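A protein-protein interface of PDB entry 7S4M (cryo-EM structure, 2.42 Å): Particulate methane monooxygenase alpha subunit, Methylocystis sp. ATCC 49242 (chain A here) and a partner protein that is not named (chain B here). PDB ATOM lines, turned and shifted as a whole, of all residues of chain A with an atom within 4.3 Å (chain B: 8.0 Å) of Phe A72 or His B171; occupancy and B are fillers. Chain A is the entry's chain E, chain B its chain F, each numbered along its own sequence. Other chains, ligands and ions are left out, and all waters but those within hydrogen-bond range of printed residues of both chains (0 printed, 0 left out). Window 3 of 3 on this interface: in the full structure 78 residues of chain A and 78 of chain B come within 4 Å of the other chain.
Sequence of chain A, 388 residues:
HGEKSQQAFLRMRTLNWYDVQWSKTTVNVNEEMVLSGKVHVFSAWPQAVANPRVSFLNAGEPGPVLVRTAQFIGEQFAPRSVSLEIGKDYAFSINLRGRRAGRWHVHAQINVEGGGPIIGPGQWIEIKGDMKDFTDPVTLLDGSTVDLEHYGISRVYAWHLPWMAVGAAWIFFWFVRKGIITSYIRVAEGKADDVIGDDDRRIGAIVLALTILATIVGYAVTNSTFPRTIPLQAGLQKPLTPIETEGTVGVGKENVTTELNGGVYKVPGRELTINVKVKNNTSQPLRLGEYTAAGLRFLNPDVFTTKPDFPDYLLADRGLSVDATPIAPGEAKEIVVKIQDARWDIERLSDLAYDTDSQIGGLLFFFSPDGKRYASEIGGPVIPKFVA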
ATOM      1  N   LEU A  57     -26.193  -7.080  28.606  1.00  0.00           N
ATOM      2  CA  LEU A  57     -26.968  -5.852  28.559  1.00  0.00           C
ATOM      3  C   LEU A  57     -28.424  -6.169  28.257  1.00  0.00           C
ATOM      4  O   LEU A  57     -28.730  -6.963  27.365  1.00  0.00           O
ATOM      5  CB  LEU A  57     -26.409  -4.907  27.499  1.00  0.00           C
ATOM      6  CG  LEU A  57     -27.283  -3.701  27.166  1.00  0.00           C
ATOM      7  CD1 LEU A  57     -27.338  -2.757  28.347  1.00  0.00           C
ATOM      8  CD2 LEU A  57     -26.765  -2.987  25.936  1.00  0.00           C
ATOM      9  N   ALA A  70     -32.266  -4.269  18.427  1.00  0.00           N
ATOM     10  CA  ALA A  70     -30.813  -4.317  18.463  1.00  0.00           C
ATOM     11  C   ALA A  70     -30.333  -3.591  19.706  1.00  0.00           C
ATOM     12  O   ALA A  70     -30.992  -2.679  20.207  1.00  0.00           O
ATOM     13  CB  ALA A  70     -30.194  -3.695  17.208  1.00  0.00           C
ATOM     14  N   GLN A  71     -29.171  -4.008  20.197  1.00  0.00           N
ATOM     15  CA  GLN A  71     -28.558  -3.350  21.338  1.00  0.00           C
ATOM     16  C   GLN A  71     -27.049  -3.387  21.169  1.00  0.00           C
ATOM     17  O   GLN A  71     -26.494  -4.358  20.651  1.00  0.00           O
ATOM     18  CB  GLN A  71     -28.970  -4.001  22.663  1.00  0.00           C
ATOM     19  CG  GLN A  71     -28.447  -5.404  22.864  1.00  0.00           C
ATOM     20  CD  GLN A  71     -28.728  -5.930  24.252  1.00  0.00           C
ATOM     21  OE1 GLN A  71     -29.626  -5.450  24.941  1.00  0.00           O
ATOM     22  NE2 GLN A  71     -27.956  -6.922  24.673  1.00  0.00           N
ATOM     23  N   PHE A  72     -26.397  -2.314  21.598  1.00  0.00           N
ATOM     24  CA  PHE A  72     -24.956  -2.191  21.472  1.00  0.00           C
ATOM     25  C   PHE A  72     -24.371  -1.772  22.809  1.00  0.00           C
ATOM     26  O   PHE A  72     -25.006  -1.037  23.568  1.00  0.00           O
ATOM     27  CB  PHE A  72     -24.563  -1.170  20.400  1.00  0.00           C
ATOM     28  CG  PHE A  72     -25.262  -1.364  19.089  1.00  0.00           C
ATOM     29  CD1 PHE A  72     -26.508  -0.810  18.869  1.00  0.00           C
ATOM     30  CD2 PHE A  72     -24.673  -2.093  18.077  1.00  0.00           C
ATOM     31  CE1 PHE A  72     -27.153  -0.984  17.667  1.00  0.00           C
ATOM     32  CE2 PHE A  72     -25.315  -2.271  16.873  1.00  0.00           C
ATOM     33  CZ  PHE A  72     -26.556  -1.715  16.668  1.00  0.00           C
ATOM     34  N   ILE A  73     -23.167  -2.254  23.095  1.00  0.00           N
ATOM     35  CA  ILE A  73     -22.399  -1.802  24.247  1.00  0.00           C
ATOM     36  C   ILE A  73     -20.924  -1.931  23.903  1.00  0.00           C
ATOM     37  O   ILE A  73     -20.512  -2.886  23.240  1.00  0.00           O
ATOM     38  CB  ILE A  73     -22.765  -2.584  25.527  1.00  0.00           C
ATOM     39  CG1 ILE A  73     -22.141  -1.916  26.751  1.00  0.00           C
ATOM     40  CG2 ILE A  73     -22.338  -4.035  25.423  1.00  0.00           C
ATOM     41  CD1 ILE A  73     -22.468  -2.600  28.051  1.00  0.00           C
ATOM     42  N   GLN A  76     -20.067  -2.287  20.155  1.00  0.00           N
ATOM     43  CA  GLN A  76     -20.220  -3.627  19.612  1.00  0.00           C
ATOM     44  C   GLN A  76     -21.680  -4.039  19.666  1.00  0.00           C
ATOM     45  O   GLN A  76     -22.366  -3.775  20.655  1.00  0.00           O
ATOM     46  CB  GLN A  76     -19.390  -4.648  20.393  1.00  0.00           C
ATOM     47  CG  GLN A  76     -18.009  -4.896  19.844  1.00  0.00           C
ATOM     48  CD  GLN A  76     -17.134  -5.620  20.839  1.00  0.00           C
ATOM     49  OE1 GLN A  76     -16.075  -5.130  21.225  1.00  0.00           O
ATOM     50  NE2 GLN A  76     -17.583  -6.790  21.277  1.00  0.00           N
ATOM     51  N   PHE A  77     -22.145  -4.696  18.609  1.00  0.00           N
ATOM     52  CA  PHE A  77     -23.454  -5.334  18.654  1.00  0.00           C
ATOM     53  C   PHE A  77     -23.401  -6.481  19.652  1.00  0.00           C
ATOM     54  O   PHE A  77     -22.575  -7.389  19.517  1.00  0.00           O
ATOM     55  CB  PHE A  77     -23.852  -5.832  17.270  1.00  0.00           C
ATOM     56  CG  PHE A  77     -25.177  -6.525  17.237  1.00  0.00           C
ATOM     57  CD1 PHE A  77     -26.300  -5.922  17.769  1.00  0.00           C
ATOM     58  CD2 PHE A  77     -25.302  -7.778  16.671  1.00  0.00           C
ATOM     59  CE1 PHE A  77     -27.520  -6.556  17.739  1.00  0.00           C
ATOM     60  CE2 PHE A  77     -26.520  -8.416  16.638  1.00  0.00           C
ATOM     61  CZ  PHE A  77     -27.631  -7.805  17.172  1.00  0.00           C
ATOM     62  N   ALA A  91     -20.419   2.798  26.799  1.00  0.00           N
ATOM     63  CA  ALA A  91     -21.601   3.424  26.229  1.00  0.00           C
ATOM     64  C   ALA A  91     -22.498   2.349  25.637  1.00  0.00           C
ATOM     65  O   ALA A  91     -22.027   1.478  24.901  1.00  0.00           O
ATOM     66  CB  ALA A  91     -21.218   4.442  25.158  1.00  0.00           C
ATOM     67  N   PHE A  92     -23.786   2.411  25.957  1.00  0.00           N
ATOM     68  CA  PHE A  92     -24.743   1.424  25.493  1.00  0.00           C
ATOM     69  C   PHE A  92     -25.933   2.116  24.849  1.00  0.00           C
ATOM     70  O   PHE A  92     -26.228   3.280  25.127  1.00  0.00           O
ATOM     71  CB  PHE A  92     -25.215   0.511  26.633  1.00  0.00           C
ATOM     72  CG  PHE A  92     -26.013   1.216  27.691  1.00  0.00           C
ATOM     73  CD1 PHE A  92     -25.385   1.833  28.755  1.00  0.00           C
ATOM     74  CD2 PHE A  92     -27.395   1.244  27.631  1.00  0.00           C
ATOM     75  CE1 PHE A  92     -26.118   2.474  29.728  1.00  0.00           C
ATOM     76  CE2 PHE A  92     -28.130   1.885  28.602  1.00  0.00           C
ATOM     77  CZ  PHE A  92     -27.491   2.500  29.651  1.00  0.00           C
ATOM     78  N   SER A  93     -26.611   1.380  23.973  1.00  0.00           N
ATOM     79  CA  SER A  93     -27.799   1.878  23.299  1.00  0.00           C
ATOM     80  C   SER A  93     -28.654   0.689  22.897  1.00  0.00           C
ATOM     81  O   SER A  93     -28.147  -0.279  22.329  1.00  0.00           O
ATOM     82  CB  SER A  93     -27.436   2.713  22.068  1.00  0.00           C
ATOM     83  OG  SER A  93     -27.367   1.902  20.910  1.00  0.00           O
ATOM     84  N   ASN A  95     -32.183  -0.395  20.856  1.00  0.00           N
ATOM     85  CA  ASN A  95     -33.232  -0.005  19.921  1.00  0.00           C
ATOM     86  C   ASN A  95     -34.485  -0.811  20.239  1.00  0.00           C
ATOM     87  O   ASN A  95     -34.565  -2.000  19.917  1.00  0.00           O
ATOM     88  CB  ASN A  95     -32.786  -0.232  18.480  1.00  0.00           C
ATOM     89  CG  ASN A  95     -31.487   0.465  18.160  1.00  0.00           C
ATOM     90  OD1 ASN A  95     -30.918   1.157  19.001  1.00  0.00           O
ATOM     91  ND2 ASN A  95     -31.009   0.289  16.935  1.00  0.00           N
ATOM     92  N   THR B 168     -30.046 -16.051   9.943  1.00  0.00           N
ATOM     93  CA  THR B 168     -30.306 -14.663   9.596  1.00  0.00           C
ATOM     94  C   THR B 168     -29.070 -13.831   9.901  1.00  0.00           C
ATOM     95  O   THR B 168     -28.237 -14.199  10.731  1.00  0.00           O
ATOM     96  CB  THR B 168     -31.506 -14.082  10.353  1.00  0.00           C
ATOM     97  OG1 THR B 168     -31.102 -13.710  11.674  1.00  0.00           O
ATOM     98  CG2 THR B 168     -32.633 -15.087  10.440  1.00  0.00           C
ATOM     99  N   GLU B 169     -28.965 -12.699   9.217  1.00  0.00           N
ATOM    100  CA  GLU B 169     -27.839 -11.789   9.367  1.00  0.00           C
ATOM    101  C   GLU B 169     -28.314 -10.556  10.123  1.00  0.00           C
ATOM    102  O   GLU B 169     -29.224  -9.858   9.668  1.00  0.00           O
ATOM    103  CB  GLU B 169     -27.273 -11.419   7.996  1.00  0.00           C
ATOM    104  CG  GLU B 169     -25.846 -10.891   7.980  1.00  0.00           C
ATOM    105  CD  GLU B 169     -25.740  -9.391   8.186  1.00  0.00           C
ATOM    106  OE1 GLU B 169     -26.718  -8.761   8.635  1.00  0.00           O
ATOM    107  OE2 GLU B 169     -24.669  -8.834   7.873  1.00  0.00           O
ATOM    108  N   GLN B 170     -27.694 -10.288  11.269  1.00  0.00           N
ATOM    109  CA  GLN B 170     -28.069  -9.169  12.128  1.00  0.00           C
ATOM    110  C   GLN B 170     -26.825  -8.351  12.432  1.00  0.00           C
ATOM    111  O   GLN B 170     -25.969  -8.785  13.209  1.00  0.00           O
ATOM    112  CB  GLN B 170     -28.721  -9.663  13.417  1.00  0.00           C
ATOM    113  CG  GLN B 170     -30.049 -10.363  13.224  1.00  0.00           C
ATOM    114  CD  GLN B 170     -31.084  -9.481  12.566  1.00  0.00           C
ATOM    115  OE1 GLN B 170     -31.461  -9.698  11.417  1.00  0.00           O
ATOM    116  NE2 GLN B 170     -31.550  -8.475  13.294  1.00  0.00           N
ATOM    117  N   HIS B 171     -26.733  -7.165  11.830  1.00  0.00           N
ATOM    118  CA  HIS B 171     -25.636  -6.232  12.080  1.00  0.00           C
ATOM    119  C   HIS B 171     -24.279  -6.893  11.853  1.00  0.00           C
ATOM    120  O   HIS B 171     -23.381  -6.833  12.696  1.00  0.00           O
ATOM    121  CB  HIS B 171     -25.732  -5.644  13.488  1.00  0.00           C
ATOM    122  CG  HIS B 171     -26.960  -4.822  13.711  1.00  0.00           C
ATOM    123  ND1 HIS B 171     -26.938  -3.445  13.740  1.00  0.00           N
ATOM    124  CD2 HIS B 171     -28.250  -5.181  13.910  1.00  0.00           C
ATOM    125  CE1 HIS B 171     -28.160  -2.991  13.949  1.00  0.00           C
ATOM    126  NE2 HIS B 171     -28.975  -4.025  14.057  1.00  0.00           N
ATOM    127  N   GLY B 172     -24.135  -7.532  10.697  1.00  0.00           N
ATOM    128  CA  GLY B 172     -22.887  -8.194  10.364  1.00  0.00           C
ATOM    129  C   GLY B 172     -22.553  -9.360  11.263  1.00  0.00           C
ATOM    130  O   GLY B 172     -21.377  -9.587  11.563  1.00  0.00           O
ATOM    131  N   GLN B 173     -23.557 -10.108  11.704  1.00  0.00           N
ATOM    132  CA  GLN B 173     -23.352 -11.229  12.606  1.00  0.00           C
ATOM    133  C   GLN B 173     -24.392 -12.298  12.315  1.00  0.00           C
ATOM    134  O   GLN B 173     -25.554 -11.984  12.050  1.00  0.00           O
ATOM    135  CB  GLN B 173     -23.443 -10.782  14.067  1.00  0.00           C
ATOM    136  CG  GLN B 173     -23.271 -11.889  15.077  1.00  0.00           C
ATOM    137  CD  GLN B 173     -23.250 -11.368  16.495  1.00  0.00           C
ATOM    138  OE1 GLN B 173     -22.724 -10.290  16.762  1.00  0.00           O
ATOM    139  NE2 GLN B 173     -23.825 -12.131  17.413  1.00  0.00           N
ATOM    140  N   LEU B 174     -23.970 -13.555  12.362  1.00  0.00           N
ATOM    141  CA  LEU B 174     -24.879 -14.660  12.110  1.00  0.00           C
ATOM    142  C   LEU B 174     -25.658 -15.010  13.369  1.00  0.00           C
ATOM    143  O   LEU B 174     -25.080 -15.201  14.441  1.00  0.00           O
ATOM    144  CB  LEU B 174     -24.111 -15.885  11.625  1.00  0.00           C
ATOM    145  CG  LEU B 174     -24.994 -17.016  11.112  1.00  0.00           C
ATOM    146  CD1 LEU B 174     -25.781 -16.564   9.902  1.00  0.00           C
ATOM    147  CD2 LEU B 174     -24.158 -18.238  10.793  1.00  0.00           C
ATOM    148  N   MET B 175     -26.978 -15.092  13.233  1.00  0.00           N
ATOM    149  CA  MET B 175     -27.842 -15.450  14.347  1.00  0.00           C
ATOM    150  C   MET B 175     -28.969 -16.326  13.826  1.00  0.00           C
ATOM    151  O   MET B 175     -29.456 -16.122  12.712  1.00  0.00           O
ATOM    152  CB  MET B 175     -28.416 -14.211  15.039  1.00  0.00           C
ATOM    153  CG  MET B 175     -27.379 -13.362  15.751  1.00  0.00           C
ATOM    154  SD  MET B 175     -28.064 -12.252  16.993  1.00  0.00           S
ATOM    155  CE  MET B 175     -29.804 -12.644  16.888  1.00  0.00           C
ATOM    156  N   LEU B 180     -32.746 -14.948  17.530  1.00  0.00           N
ATOM    157  CA  LEU B 180     -33.379 -13.657  17.292  1.00  0.00           C
ATOM    158  C   LEU B 180     -34.676 -13.526  18.077  1.00  0.00           C
ATOM    159  O   LEU B 180     -34.966 -12.463  18.634  1.00  0.00           O
ATOM    160  CB  LEU B 180     -33.626 -13.470  15.799  1.00  0.00           C
ATOM    161  CG  LEU B 180     -33.930 -12.051  15.334  1.00  0.00           C
ATOM    162  CD1 LEU B 180     -32.918 -11.084  15.904  1.00  0.00           C
ATOM    163  CD2 LEU B 180     -33.915 -12.003  13.824  1.00  0.00           C
ATOM    164  N   PHE B 183     -33.842 -12.913  21.597  1.00  0.00           N
ATOM    165  CA  PHE B 183     -33.268 -11.585  21.770  1.00  0.00           C
ATOM    166  C   PHE B 183     -34.324 -10.498  21.625  1.00  0.00           C
ATOM    167  O   PHE B 183     -34.279  -9.485  22.332  1.00  0.00           O
ATOM    168  CB  PHE B 183     -32.142 -11.377  20.762  1.00  0.00           C
ATOM    169  CG  PHE B 183     -31.560 -10.001  20.783  1.00  0.00           C
ATOM    170  CD1 PHE B 183     -30.848  -9.554  21.878  1.00  0.00           C
ATOM    171  CD2 PHE B 183     -31.712  -9.158  19.701  1.00  0.00           C
ATOM    172  CE1 PHE B 183     -30.309  -8.291  21.897  1.00  0.00           C
ATOM    173  CE2 PHE B 183     -31.174  -7.893  19.715  1.00  0.00           C
ATOM    174  CZ  PHE B 183     -30.471  -7.460  20.814  1.00  0.00           C
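O of Leu A57 lies within hydrogen-bond range of NE2 of Gln A71, at 2.8 Å. The backbone NH of Asn A95 lies within hydrogen-bond range of the backbone carbonyl oxygen of Ala A70, at 2.7 Å. The backbone carbonyl oxygen (O) of Ser A93 sits at hydrogen-bond distance from the backbone NH (N) of Phe A72, 2.8 Å away.
Among the printed residues, merely in contact across the chains: Ala A70 with His B171 (3.4 Å), Ala A70 with Phe B183 (3.8 Å), Gln A71 with Phe B183 (3.5 Å), Phe A72 with His B171 (3.4 Å), Phe A77 with Gln B170 (3.5 Å), Phe A77 with His B171 (3.9 Å) and Phe A77 with Gln B173 (3.6 Å).
Of the printed residues of chain B, Ala A70 touches His B171 (3.4 Å) and Phe B183 (3.8 Å). Phe A72 touches just one residue of chain B: His B171 (3.4 Å). Of the printed residues of chain B, Phe A77 touches Gln B170, His B171 and Gln B173. Phe A92 touches none of the printed residues of chain B. Of chain A, only Ala A70 (3.4 Å), Phe A72 (3.4 Å) and Phe A77 (3.9 Å) come within 4 Å of His B171. Of the printed residues of chain A, Phe B183 touches Ala A70 and Gln A71. The nearest printed residue of chain A that does not touch His B171 is Asn A95 (5.3 Å). The nearest printed residue of chain A that does not touch Gln B170 is Ala A70 (6.3 Å).
Of the 11 printed residues of chain A, 4 touch a printed residue of chain B. Among the printed residues, no Asp or Glu carboxylate lies within 4 Å of a Lys or Arg side-chain nitrogen of the other chain.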
